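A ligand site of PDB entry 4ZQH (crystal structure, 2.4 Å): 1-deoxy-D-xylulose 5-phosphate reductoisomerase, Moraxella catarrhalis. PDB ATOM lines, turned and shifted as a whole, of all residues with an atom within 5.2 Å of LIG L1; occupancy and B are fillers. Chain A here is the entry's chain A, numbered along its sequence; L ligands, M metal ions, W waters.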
ATOM      1  N   GLY A  30     -13.032  14.997   5.196  1.00  0.00           N
ATOM      2  CA  GLY A  30     -12.519  15.632   3.989  1.00  0.00           C
ATOM      3  C   GLY A  30     -12.534  14.619   2.872  1.00  0.00           C
ATOM      4  O   GLY A  30     -11.649  14.609   2.050  1.00  0.00           O
ATOM      5  N   ALA A  31     -13.576  13.795   2.848  1.00  0.00           N
ATOM      6  CA  ALA A  31     -13.662  12.661   1.939  1.00  0.00           C
ATOM      7  C   ALA A  31     -13.884  13.062   0.497  1.00  0.00           C
ATOM      8  O   ALA A  31     -13.654  12.256  -0.369  1.00  0.00           O
ATOM      9  CB  ALA A  31     -14.777  11.725   2.385  1.00  0.00           C
ATOM     10  N   THR A  32     -14.345  14.266   0.264  1.00  0.00           N
ATOM     11  CA  THR A  32     -14.687  14.707  -1.071  1.00  0.00           C
ATOM     12  C   THR A  32     -13.519  15.365  -1.807  1.00  0.00           C
ATOM     13  O   THR A  32     -13.609  15.623  -3.016  1.00  0.00           O
ATOM     14  CB  THR A  32     -15.866  15.753  -1.049  1.00  0.00           C
ATOM     15  OG1 THR A  32     -15.557  16.836  -0.150  1.00  0.00           O
ATOM     16  CG2 THR A  32     -17.186  15.099  -0.648  1.00  0.00           C
ATOM     17  N   GLY A  33     -12.452  15.674  -1.080  1.00  0.00           N
ATOM     18  CA  GLY A  33     -11.278  16.340  -1.645  1.00  0.00           C
ATOM     19  C   GLY A  33     -10.167  15.417  -2.153  1.00  0.00           C
ATOM     20  O   GLY A  33     -10.329  14.179  -2.297  1.00  0.00           O
ATOM     21  N   SER A  34      -9.040  16.042  -2.450  1.00  0.00           N
ATOM     22  CA  SER A  34      -7.906  15.370  -3.086  1.00  0.00           C
ATOM     23  C   SER A  34      -7.375  14.172  -2.303  1.00  0.00           C
ATOM     24  O   SER A  34      -7.239  13.064  -2.832  1.00  0.00           O
ATOM     25  CB  SER A  34      -6.812  16.395  -3.275  1.00  0.00           C
ATOM     26  OG  SER A  34      -5.668  15.740  -3.656  1.00  0.00           O
ATOM     27  N   ILE A  35      -7.124  14.412  -1.027  1.00  0.00           N
ATOM     28  CA  ILE A  35      -6.643  13.374  -0.154  1.00  0.00           C
ATOM     29  C   ILE A  35      -7.737  12.349   0.035  1.00  0.00           C
ATOM     30  O   ILE A  35      -7.450  11.137   0.094  1.00  0.00           O
ATOM     31  CB  ILE A  35      -6.144  13.972   1.174  1.00  0.00           C
ATOM     32  CG1 ILE A  35      -4.798  14.706   0.952  1.00  0.00           C
ATOM     33  CG2 ILE A  35      -6.011  12.925   2.268  1.00  0.00           C
ATOM     34  CD1 ILE A  35      -3.592  13.821   0.696  1.00  0.00           C
ATOM     35  N   GLY A  36      -8.983  12.836   0.117  1.00  0.00           N
ATOM     36  CA  GLY A  36     -10.171  11.953   0.086  1.00  0.00           C
ATOM     37  C   GLY A  36     -10.180  10.930  -1.050  1.00  0.00           C
ATOM     38  O   GLY A  36     -10.399   9.750  -0.833  1.00  0.00           O
ATOM     39  N   THR A  56     -17.157  12.670   5.338  1.00  0.00           N
ATOM     40  CA  THR A  56     -17.588  14.032   5.432  1.00  0.00           C
ATOM     41  C   THR A  56     -17.163  14.847   4.239  1.00  0.00           C
ATOM     42  O   THR A  56     -16.149  14.595   3.659  1.00  0.00           O
ATOM     43  CB  THR A  56     -17.034  14.741   6.695  1.00  0.00           C
ATOM     44  OG1 THR A  56     -15.784  15.436   6.409  1.00  0.00           O
ATOM     45  CG2 THR A  56     -16.838  13.773   7.821  1.00  0.00           C
ATOM     46  N   GLY A  57     -17.963  15.854   3.913  1.00  0.00           N
ATOM     47  CA  GLY A  57     -17.682  16.809   2.873  1.00  0.00           C
ATOM     48  C   GLY A  57     -18.304  18.110   3.314  1.00  0.00           C
ATOM     49  O   GLY A  57     -18.946  18.147   4.355  1.00  0.00           O
ATOM     50  N   PHE A  58     -18.114  19.174   2.549  1.00  0.00           N
ATOM     51  CA  PHE A  58     -18.610  20.485   2.896  1.00  0.00           C
ATOM     52  C   PHE A  58     -19.540  20.967   1.776  1.00  0.00           C
ATOM     53  O   PHE A  58     -20.748  20.893   1.921  1.00  0.00           O
ATOM     54  CB  PHE A  58     -17.443  21.466   3.152  1.00  0.00           C
ATOM     55  CG  PHE A  58     -17.841  22.744   3.868  1.00  0.00           C
ATOM     56  CD1 PHE A  58     -18.233  22.718   5.203  1.00  0.00           C
ATOM     57  CD2 PHE A  58     -17.802  23.978   3.212  1.00  0.00           C
ATOM     58  CE1 PHE A  58     -18.619  23.876   5.849  1.00  0.00           C
ATOM     59  CE2 PHE A  58     -18.168  25.146   3.865  1.00  0.00           C
ATOM     60  CZ  PHE A  58     -18.580  25.090   5.192  1.00  0.00           C
ATOM     61  N   SER A  59     -18.983  21.421   0.656  1.00  0.00           N
ATOM     62  CA  SER A  59     -19.754  22.022  -0.399  1.00  0.00           C
ATOM     63  C   SER A  59     -20.177  21.032  -1.494  1.00  0.00           C
ATOM     64  O   SER A  59     -21.175  21.262  -2.194  1.00  0.00           O
ATOM     65  CB  SER A  59     -18.944  23.161  -0.999  1.00  0.00           C
ATOM     66  OG  SER A  59     -18.049  22.652  -1.957  1.00  0.00           O
ATOM     67  N   ARG A  60     -19.460  19.918  -1.649  1.00  0.00           N
ATOM     68  CA  ARG A  60     -19.750  18.957  -2.730  1.00  0.00           C
ATOM     69  C   ARG A  60     -20.740  17.900  -2.285  1.00  0.00           C
ATOM     70  O   ARG A  60     -20.364  16.726  -2.049  1.00  0.00           O
ATOM     71  CB  ARG A  60     -18.463  18.363  -3.316  1.00  0.00           C
ATOM     72  CG  ARG A  60     -17.717  19.384  -4.169  1.00  0.00           C
ATOM     73  CD  ARG A  60     -16.468  18.831  -4.799  1.00  0.00           C
ATOM     74  NE  ARG A  60     -15.312  19.129  -3.990  1.00  0.00           N
ATOM     75  CZ  ARG A  60     -14.065  18.753  -4.261  1.00  0.00           C
ATOM     76  NH1 ARG A  60     -13.803  18.049  -5.347  1.00  0.00           N
ATOM     77  NH2 ARG A  60     -13.086  19.072  -3.427  1.00  0.00           N
ATOM     78  N   LEU A 106     -18.702  16.802  12.853  1.00  0.00           N
ATOM     79  CA  LEU A 106     -17.313  16.384  12.787  1.00  0.00           C
ATOM     80  C   LEU A 106     -16.842  15.893  14.144  1.00  0.00           C
ATOM     81  O   LEU A 106     -16.228  14.838  14.238  1.00  0.00           O
ATOM     82  CB  LEU A 106     -16.431  17.542  12.285  1.00  0.00           C
ATOM     83  CG  LEU A 106     -16.866  18.153  10.952  1.00  0.00           C
ATOM     84  CD1 LEU A 106     -15.921  19.260  10.545  1.00  0.00           C
ATOM     85  CD2 LEU A 106     -16.983  17.080   9.885  1.00  0.00           C
ATOM     86  N   ALA A 121      -8.378  14.899   6.916  1.00  0.00           N
ATOM     87  CA  ALA A 121      -7.985  15.475   5.627  1.00  0.00           C
ATOM     88  C   ALA A 121      -8.820  16.652   5.248  1.00  0.00           C
ATOM     89  O   ALA A 121      -8.916  16.990   4.058  1.00  0.00           O
ATOM     90  CB  ALA A 121      -8.029  14.432   4.501  1.00  0.00           C
ATOM     91  N   ILE A 122      -9.401  17.309   6.248  1.00  0.00           N
ATOM     92  CA  ILE A 122     -10.004  18.634   6.032  1.00  0.00           C
ATOM     93  C   ILE A 122      -8.888  19.639   5.808  1.00  0.00           C
ATOM     94  O   ILE A 122      -7.857  19.569   6.415  1.00  0.00           O
ATOM     95  CB  ILE A 122     -10.890  19.072   7.214  1.00  0.00           C
ATOM     96  CG1 ILE A 122     -12.088  18.138   7.338  1.00  0.00           C
ATOM     97  CG2 ILE A 122     -11.410  20.506   7.005  1.00  0.00           C
ATOM     98  CD1 ILE A 122     -12.943  18.435   8.551  1.00  0.00           C
ATOM     99  N   VAL A 123      -9.094  20.566   4.900  1.00  0.00           N
ATOM    100  CA  VAL A 123      -8.101  21.632   4.698  1.00  0.00           C
ATOM    101  C   VAL A 123      -8.253  22.786   5.686  1.00  0.00           C
ATOM    102  O   VAL A 123      -9.345  23.160   6.061  1.00  0.00           O
ATOM    103  CB  VAL A 123      -8.161  22.201   3.279  1.00  0.00           C
ATOM    104  CG1 VAL A 123      -9.475  22.930   3.033  1.00  0.00           C
ATOM    105  CG2 VAL A 123      -6.991  23.146   3.051  1.00  0.00           C
ATOM    106  N   GLY A 124      -7.105  23.317   6.113  1.00  0.00           N
ATOM    107  CA  GLY A 124      -7.031  24.582   6.839  1.00  0.00           C
ATOM    108  C   GLY A 124      -7.427  24.465   8.277  1.00  0.00           C
ATOM    109  O   GLY A 124      -7.630  23.343   8.795  1.00  0.00           O
ATOM    110  N   ALA A 126     -10.141  24.902   9.630  1.00  0.00           N
ATOM    111  CA  ALA A 126     -11.436  24.209   9.733  1.00  0.00           C
ATOM    112  C   ALA A 126     -11.330  22.785  10.267  1.00  0.00           C
ATOM    113  O   ALA A 126     -12.301  22.267  10.827  1.00  0.00           O
ATOM    114  CB  ALA A 126     -12.122  24.202   8.376  1.00  0.00           C
ATOM    115  N   ALA A 144      -3.335  14.216   7.520  1.00  0.00           N
ATOM    116  CA  ALA A 144      -2.976  15.001   6.368  1.00  0.00           C
ATOM    117  C   ALA A 144      -3.072  16.469   6.722  1.00  0.00           C
ATOM    118  O   ALA A 144      -2.317  17.298   6.218  1.00  0.00           O
ATOM    119  CB  ALA A 144      -3.933  14.684   5.215  1.00  0.00           C
ATOM    120  N   ASN A 145      -4.028  16.799   7.574  1.00  0.00           N
ATOM    121  CA  ASN A 145      -4.422  18.190   7.808  1.00  0.00           C
ATOM    122  C   ASN A 145      -3.364  18.939   8.606  1.00  0.00           C
ATOM    123  O   ASN A 145      -3.431  18.982   9.850  1.00  0.00           O
ATOM    124  CB  ASN A 145      -5.779  18.194   8.525  1.00  0.00           C
ATOM    125  CG  ASN A 145      -6.216  19.573   8.986  1.00  0.00           C
ATOM    126  OD1 ASN A 145      -6.839  19.680  10.034  1.00  0.00           O
ATOM    127  ND2 ASN A 145      -5.916  20.617   8.206  1.00  0.00           N
ATOM    128  N   LYS A 146      -2.387  19.488   7.902  1.00  0.00           N
ATOM    129  CA  LYS A 146      -1.182  20.027   8.538  1.00  0.00           C
ATOM    130  C   LYS A 146      -1.434  21.374   9.261  1.00  0.00           C
ATOM    131  O   LYS A 146      -0.727  21.734  10.215  1.00  0.00           O
ATOM    132  CB  LYS A 146      -0.034  20.146   7.530  1.00  0.00           C
ATOM    133  CG  LYS A 146      -0.169  21.284   6.541  1.00  0.00           C
ATOM    134  CD  LYS A 146       0.865  21.205   5.431  1.00  0.00           C
ATOM    135  CE  LYS A 146       0.529  20.073   4.450  1.00  0.00           C
ATOM    136  NZ  LYS A 146       1.449  20.005   3.270  1.00  0.00           N
ATOM    137  N   GLU A 147      -2.445  22.102   8.832  1.00  0.00           N
ATOM    138  CA  GLU A 147      -2.770  23.360   9.457  1.00  0.00           C
ATOM    139  C   GLU A 147      -3.204  23.174  10.913  1.00  0.00           C
ATOM    140  O   GLU A 147      -3.003  24.067  11.722  1.00  0.00           O
ATOM    141  CB  GLU A 147      -3.843  24.092   8.649  1.00  0.00           C
ATOM    142  CG  GLU A 147      -3.347  24.518   7.266  1.00  0.00           C
ATOM    143  CD  GLU A 147      -3.628  23.506   6.156  1.00  0.00           C
ATOM    144  OE1 GLU A 147      -3.863  22.306   6.452  1.00  0.00           O
ATOM    145  OE2 GLU A 147      -3.651  23.914   4.970  1.00  0.00           O
ATOM    146  N   ASP A 171       0.999  13.333   5.504  1.00  0.00           N
ATOM    147  CA  ASP A 171       1.814  14.273   4.758  1.00  0.00           C
ATOM    148  C   ASP A 171       3.055  13.489   4.272  1.00  0.00           C
ATOM    149  O   ASP A 171       3.683  12.700   5.026  1.00  0.00           O
ATOM    150  CB  ASP A 171       2.178  15.506   5.623  1.00  0.00           C
ATOM    151  CG  ASP A 171       2.382  16.770   4.790  1.00  0.00           C
ATOM    152  OD1 ASP A 171       2.426  16.657   3.581  1.00  0.00           O
ATOM    153  OD2 ASP A 171       2.480  17.886   5.344  1.00  0.00           O
ATOM    154  N   SER A 172       3.376  13.665   2.999  1.00  0.00           N
ATOM    155  CA  SER A 172       4.371  12.853   2.336  1.00  0.00           C
ATOM    156  C   SER A 172       5.750  12.911   3.039  1.00  0.00           C
ATOM    157  O   SER A 172       6.389  11.875   3.311  1.00  0.00           O
ATOM    158  CB  SER A 172       4.472  13.312   0.875  1.00  0.00           C
ATOM    159  OG  SER A 172       5.407  12.551   0.172  1.00  0.00           O
ATOM    160  N   TRP A 233       2.525  17.066  -8.908  1.00  0.00           N
ATOM    161  CA  TRP A 233       1.485  16.666  -7.949  1.00  0.00           C
ATOM    162  C   TRP A 233       0.148  17.227  -8.414  1.00  0.00           C
ATOM    163  O   TRP A 233       0.088  18.321  -8.967  1.00  0.00           O
ATOM    164  CB  TRP A 233       1.748  17.266  -6.573  1.00  0.00           C
ATOM    165  CG  TRP A 233       2.871  16.764  -5.811  1.00  0.00           C
ATOM    166  CD1 TRP A 233       4.063  17.366  -5.642  1.00  0.00           C
ATOM    167  CD2 TRP A 233       2.921  15.569  -5.040  1.00  0.00           C
ATOM    168  NE1 TRP A 233       4.875  16.616  -4.837  1.00  0.00           N
ATOM    169  CE2 TRP A 233       4.188  15.508  -4.449  1.00  0.00           C
ATOM    170  CE3 TRP A 233       2.023  14.533  -4.807  1.00  0.00           C
ATOM    171  CZ2 TRP A 233       4.577  14.430  -3.649  1.00  0.00           C
ATOM    172  CZ3 TRP A 233       2.396  13.495  -3.991  1.00  0.00           C
ATOM    173  CH2 TRP A 233       3.676  13.444  -3.438  1.00  0.00           C
ATOM    174  N   SER A 234      -0.925  16.481  -8.185  1.00  0.00           N
ATOM    175  CA  SER A 234      -2.266  17.001  -8.387  1.00  0.00           C
ATOM    176  C   SER A 234      -2.946  17.096  -7.011  1.00  0.00           C
ATOM    177  O   SER A 234      -3.164  16.073  -6.351  1.00  0.00           O
ATOM    178  CB  SER A 234      -3.049  16.101  -9.317  1.00  0.00           C
ATOM    179  OG  SER A 234      -4.244  16.751  -9.702  1.00  0.00           O
ATOM    180  N   MET A 235      -3.246  18.315  -6.558  1.00  0.00           N
ATOM    181  CA  MET A 235      -3.700  18.479  -5.191  1.00  0.00           C
ATOM    182  C   MET A 235      -4.849  19.475  -5.074  1.00  0.00           C
ATOM    183  O   MET A 235      -5.329  20.004  -6.054  1.00  0.00           O
ATOM    184  CB  MET A 235      -2.543  18.956  -4.318  1.00  0.00           C
ATOM    185  CG  MET A 235      -1.212  18.331  -4.625  1.00  0.00           C
ATOM    186  SD  MET A 235       0.136  19.137  -3.750  1.00  0.00           S
ATOM    187  CE  MET A 235       0.398  20.543  -4.848  1.00  0.00           C
ATOM    188  N   GLY A 236      -5.284  19.709  -3.826  1.00  0.00           N
ATOM    189  CA  GLY A 236      -6.261  20.723  -3.558  1.00  0.00           C
ATOM    190  C   GLY A 236      -5.725  22.063  -3.963  1.00  0.00           C
ATOM    191  O   GLY A 236      -4.532  22.217  -4.187  1.00  0.00           O
ATOM    192  N   GLN A 237      -6.631  23.029  -4.071  1.00  0.00           N
ATOM    193  CA  GLN A 237      -6.287  24.399  -4.436  1.00  0.00           C
ATOM    194  C   GLN A 237      -5.300  25.078  -3.492  1.00  0.00           C
ATOM    195  O   GLN A 237      -4.360  25.725  -3.956  1.00  0.00           O
ATOM    196  CB  GLN A 237      -7.544  25.237  -4.503  1.00  0.00           C
ATOM    197  CG  GLN A 237      -8.237  25.160  -5.842  1.00  0.00           C
ATOM    198  CD  GLN A 237      -9.331  26.207  -5.949  1.00  0.00           C
ATOM    199  OE1 GLN A 237     -10.102  26.445  -4.993  1.00  0.00           O
ATOM    200  NE2 GLN A 237      -9.400  26.855  -7.118  1.00  0.00           N
ATOM    201  N   ILE A 239      -3.125  23.999  -1.000  1.00  0.00           N
ATOM    202  CA  ILE A 239      -1.797  23.431  -0.918  1.00  0.00           C
ATOM    203  C   ILE A 239      -1.068  23.655  -2.245  1.00  0.00           C
ATOM    204  O   ILE A 239       0.135  23.778  -2.275  1.00  0.00           O
ATOM    205  CB  ILE A 239      -1.818  21.928  -0.542  1.00  0.00           C
ATOM    206  CG1 ILE A 239      -0.417  21.428  -0.235  1.00  0.00           C
ATOM    207  CG2 ILE A 239      -2.408  21.069  -1.638  1.00  0.00           C
ATOM    208  CD1 ILE A 239      -0.402  20.163   0.608  1.00  0.00           C
ATOM    209  N   MET A 297       0.177  10.404  -3.417  1.00  0.00           N
ATOM    210  CA  MET A 297      -0.169  10.288  -2.004  1.00  0.00           C
ATOM    211  C   MET A 297      -0.730   8.938  -1.617  1.00  0.00           C
ATOM    212  O   MET A 297      -0.963   8.692  -0.452  1.00  0.00           O
ATOM    213  CB  MET A 297      -1.178  11.361  -1.608  1.00  0.00           C
ATOM    214  CG  MET A 297      -0.670  12.809  -1.738  1.00  0.00           C
ATOM    215  SD  MET A 297       0.834  13.114  -0.803  1.00  0.00           S
ATOM    216  CE  MET A 297       0.338  12.676   0.864  1.00  0.00           C
HETATM  217  P1  LIG L   1      -9.158  19.793  -0.902  1.00  0.00           P
HETATM  218  O1  LIG L   1      -9.405  21.257  -1.167  1.00  0.00           O
HETATM  219  O2  LIG L   1      -9.144  18.811  -2.040  1.00  0.00           O
HETATM  220  O3  LIG L   1     -10.164  19.123   0.141  1.00  0.00           O
HETATM  221  C1  LIG L   1     -10.632  19.768   1.305  1.00  0.00           C
HETATM  222  C2  LIG L   1     -11.596  18.839   2.055  1.00  0.00           C
HETATM  223  O4  LIG L   1     -12.063  19.454   3.283  1.00  0.00           O
HETATM  224  C3  LIG L   1     -12.833  18.571   1.209  1.00  0.00           C
HETATM  225  O5  LIG L   1     -13.429  17.333   1.574  1.00  0.00           O
HETATM  226  C4  LIG L   1     -13.734  19.754   1.567  1.00  0.00           C
HETATM  227  O6  LIG L   1     -15.095  19.505   1.217  1.00  0.00           O
HETATM  228  C5  LIG L   1     -13.424  19.883   3.073  1.00  0.00           C
HETATM  229  N1  LIG L   1     -13.615  21.281   3.585  1.00  0.00           N
HETATM  230  C6  LIG L   1     -13.222  22.423   2.972  1.00  0.00           C
HETATM  231  N2  LIG L   1     -13.574  23.490   3.703  1.00  0.00           N
HETATM  232  C7  LIG L   1     -14.190  23.027   4.813  1.00  0.00           C
HETATM  233  C8  LIG L   1     -14.803  23.643   6.003  1.00  0.00           C
HETATM  234  N3  LIG L   1     -14.779  24.992   6.122  1.00  0.00           N
HETATM  235  N4  LIG L   1     -15.352  22.840   6.934  1.00  0.00           N
HETATM  236  C9  LIG L   1     -15.331  21.501   6.777  1.00  0.00           C
HETATM  237  N5  LIG L   1     -14.813  20.874   5.713  1.00  0.00           N
HETATM  238  C10 LIG L   1     -14.233  21.587   4.719  1.00  0.00           C
HETATM  239  O7  LIG L   1      -7.738  19.810  -0.133  1.00  0.00           O
HETATM  240  P2  LIG L   1      -6.670  18.623  -0.045  1.00  0.00           P
HETATM  241  O8  LIG L   1      -7.316  17.236   0.060  1.00  0.00           O
HETATM  242  O9  LIG L   1      -5.633  18.984  -1.058  1.00  0.00           O
HETATM  243  O10 LIG L   1      -5.982  18.901   1.345  1.00  0.00           O
HETATM  244  C11 LIG L   1      -6.520  18.276   2.501  1.00  0.00           C
HETATM  245  C12 LIG L   1      -5.479  18.403   3.587  1.00  0.00           C
HETATM  246  O11 LIG L   1      -4.387  17.539   3.294  1.00  0.00           O
HETATM  247  C13 LIG L   1      -4.896  19.789   3.672  1.00  0.00           C
HETATM  248  O12 LIG L   1      -4.730  20.020   5.078  1.00  0.00           O
HETATM  249  C14 LIG L   1      -3.565  19.696   2.966  1.00  0.00           C
HETATM  250  O13 LIG L   1      -2.636  20.637   3.523  1.00  0.00           O
HETATM  251  C15 LIG L   1      -3.165  18.242   3.220  1.00  0.00           C
HETATM  252  N6  LIG L   1      -2.331  17.624   2.188  1.00  0.00           N
HETATM  253  C16 LIG L   1      -2.797  17.404   0.957  1.00  0.00           C
HETATM  254  C17 LIG L   1      -2.031  16.826  -0.056  1.00  0.00           C
HETATM  255  C18 LIG L   1      -2.608  16.538  -1.430  1.00  0.00           C
HETATM  256  O14 LIG L   1      -3.697  16.957  -1.823  1.00  0.00           O
HETATM  257  N7  LIG L   1      -1.901  15.769  -2.241  1.00  0.00           N
HETATM  258  C19 LIG L   1      -0.611  16.416   0.227  1.00  0.00           C
HETATM  259  C20 LIG L   1      -0.220  16.705   1.591  1.00  0.00           C
HETATM  260  C21 LIG L   1      -1.093  17.274   2.515  1.00  0.00           C
HETATM  261  P3  LIG L   1     -15.671  20.057  -0.205  1.00  0.00           P
HETATM  262  O15 LIG L   1     -14.530  19.877  -1.165  1.00  0.00           O
HETATM  263  O16 LIG L   1     -16.843  19.125  -0.411  1.00  0.00           O
HETATM  264  O17 LIG L   1     -15.972  21.518   0.006  1.00  0.00           O
HETATM  265  O1  LG2 L   2       3.054  18.623   0.542  1.00  0.00           O
HETATM  266  N1  LG2 L   2       2.961  17.720  -0.495  1.00  0.00           N
HETATM  267  C1  LG2 L   2       2.957  16.469  -0.291  1.00  0.00           C
HETATM  268  O2  LG2 L   2       3.115  16.040   0.835  1.00  0.00           O
HETATM  269  C2  LG2 L   2       3.002  18.278  -1.839  1.00  0.00           C
HETATM  270  C3  LG2 L   2       4.438  18.820  -1.895  1.00  0.00           C
HETATM  271  C4  LG2 L   2       4.609  19.956  -2.887  1.00  0.00           C
HETATM  272  P1  LG2 L   2       6.076  20.904  -2.425  1.00  0.00           P
HETATM  273  O3  LG2 L   2       7.279  20.057  -2.449  1.00  0.00           O
HETATM  274  O4  LG2 L   2       6.234  22.030  -3.538  1.00  0.00           O
HETATM  275  O5  LG2 L   2       5.933  21.435  -0.910  1.00  0.00           O
HETATM  276 MG    MG M   1       3.826  17.518   2.217  1.00  0.00          MG
HETATM  277  O   HOH W   1      -5.324  21.637  -0.247  1.00  0.00           O
HETATM  278  O   HOH W   2      -7.766  23.074  -0.602  1.00  0.00           O
HETATM  279  O   HOH W   3     -14.122  22.063  -2.558  1.00  0.00           O
HETATM  280  O   HOH W   4      -2.495  14.687  -4.405  1.00  0.00           O
HETATM  281  O   HOH W   5      -9.211  15.553   0.833  1.00  0.00           O
HETATM  282  O   HOH W   6      -2.289  23.101   2.669  1.00  0.00           O
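The side-chain hydroxyl (OG1) of Thr 32 is in hydrogen-bond range of an oxygen (O16) of LIG L1, 2.6 Å away.
An oxygen (O12) of LIG L1 sits close to the side-chain amide nitrogen (ND2) of Asn 145.
N of Ser 172 sits close to O2 of LG2 L2 (3.2 Å).
The backbone NH of Gly 33 lies within hydrogen-bond range of an oxygen (O5) of LIG L1.
OE1 of Glu 147 lies within hydrogen-bond range of O12 of LIG L1.
O17 of LIG L1 lies within hydrogen-bond range of OG of Ser 59 (3.1 Å).
The backbone NH (N) of Gly 236 is in hydrogen-bond range of an oxygen (O9) of LIG L1.
An oxygen (O12) of LIG L1 lies within hydrogen-bond range of the backbone carbonyl oxygen of Ile 122 (3.4 Å).
The side-chain amino group (NZ) of Lys 146 lies close to an oxygen (O1) of LG2 L2, at 3.5 Å.
OG of Ser 34 is in hydrogen-bond range of O14 of LIG L1.
O of Gly 30 lies close to O5 of LIG L1.
O8 of LIG L1 sits at hydrogen-bond distance from N of Ile 35 (3.0 Å).
O16 of LIG L1 lies within hydrogen-bond range of N of Arg 60, 3.0 Å away.
N of Ser 59 is in hydrogen-bond range of O17 of LIG L1 (3.1 Å).
N of Ser 34 sits at hydrogen-bond distance from O2 of LIG L1 (2.8 Å).
The guanidinium group of Arg 60 lies within salt-bridge range of an oxygen (O15) of LIG L1 (2.8 Å).
O5 of LIG L1 sits at hydrogen-bond distance from N of Thr 32 (3.5 Å).
N of Phe 58 sits at hydrogen-bond distance from O16 of LIG L1 (3.2 Å).
O of Thr 32 lies within hydrogen-bond range of NH1 of Arg 60 (3.4 Å).
The side-chain carboxylate of Glu 147 is in hydrogen-bond range of the backbone NH of Gly 124, at 3.4 Å.
The side-chain carboxylate (OD2) of Asp 171 lies within salt-bridge range of the side-chain amino group (NZ) of Lys 146 (3.1 Å).
OE1 of Glu 147 is in hydrogen-bond range of ND2 of Asn 145 (3.2 Å).
ND2 of Asn 145 lies within hydrogen-bond range of O of Gly 124 (3.3 Å).
N of Gly 30 sits at hydrogen-bond distance from OG1 of Thr 56, 3.0 Å away.
O of Thr 56 is in hydrogen-bond range of N of Ala 31 (2.8 Å).
The side-chain amide nitrogen of Asn 145 lies within hydrogen-bond range of the backbone carbonyl oxygen of Ile 122.
N of Ala 31 touches O5 of LIG L1 (3.8 Å).
Ala 121 touches LIG L1 (O to C11, 3.1 Å).
Val 123 touches LIG L1.
Ala 126 touches LIG L1.
Ala 144 touches LIG L1.
Lys 146 touches LIG L1.
OD1 of Asp 171 touches C20 of LIG L1 (3.3 Å).
Met 235 touches LIG L1.
Ile 239 touches LIG L1.
CG of Met 297 touches N7 of LIG L1 (3.2 Å).
Hydrophobic or aromatic side chains within 4 Å of LIG L1: Ile 35, Phe 58, Ile 122, Val 123, Ala 126, Ala 144, Met 235, Ile 239 and Met 297.
22 residues have an atom within 4 Å of LIG L1: Gly 30, Ala 31, Thr 32, Gly 33, Ser 34, Ile 35, Phe 58, Ser 59, Arg 60, Ala 121, Ile 122, Val 123, Ala 126, Ala 144, Asn 145, Lys 146, Glu 147, Asp 171, Met 235, Gly 236, Ile 239 and Met 297.
The nearest printed residue that does not touch LIG L1 is Gly 57 (4.1 Å).
Water W4 lies within hydrogen-bond range of O of Ser 234 (2.5 Å), N7 of LIG L1 (2.5 Å) and OG of Ser 34 (3.4 Å).
Water W3 lies within hydrogen-bond range of O15 of LIG L1 (2.6 Å) and NH2 of Arg 60 (3.3 Å).
Water W6 lies within hydrogen-bond range of O13 of LIG L1 (2.6 Å) and OE2 of Glu 147 (2.8 Å).
Water W1 bridges O9 of LIG L1 and N of Ile 239.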
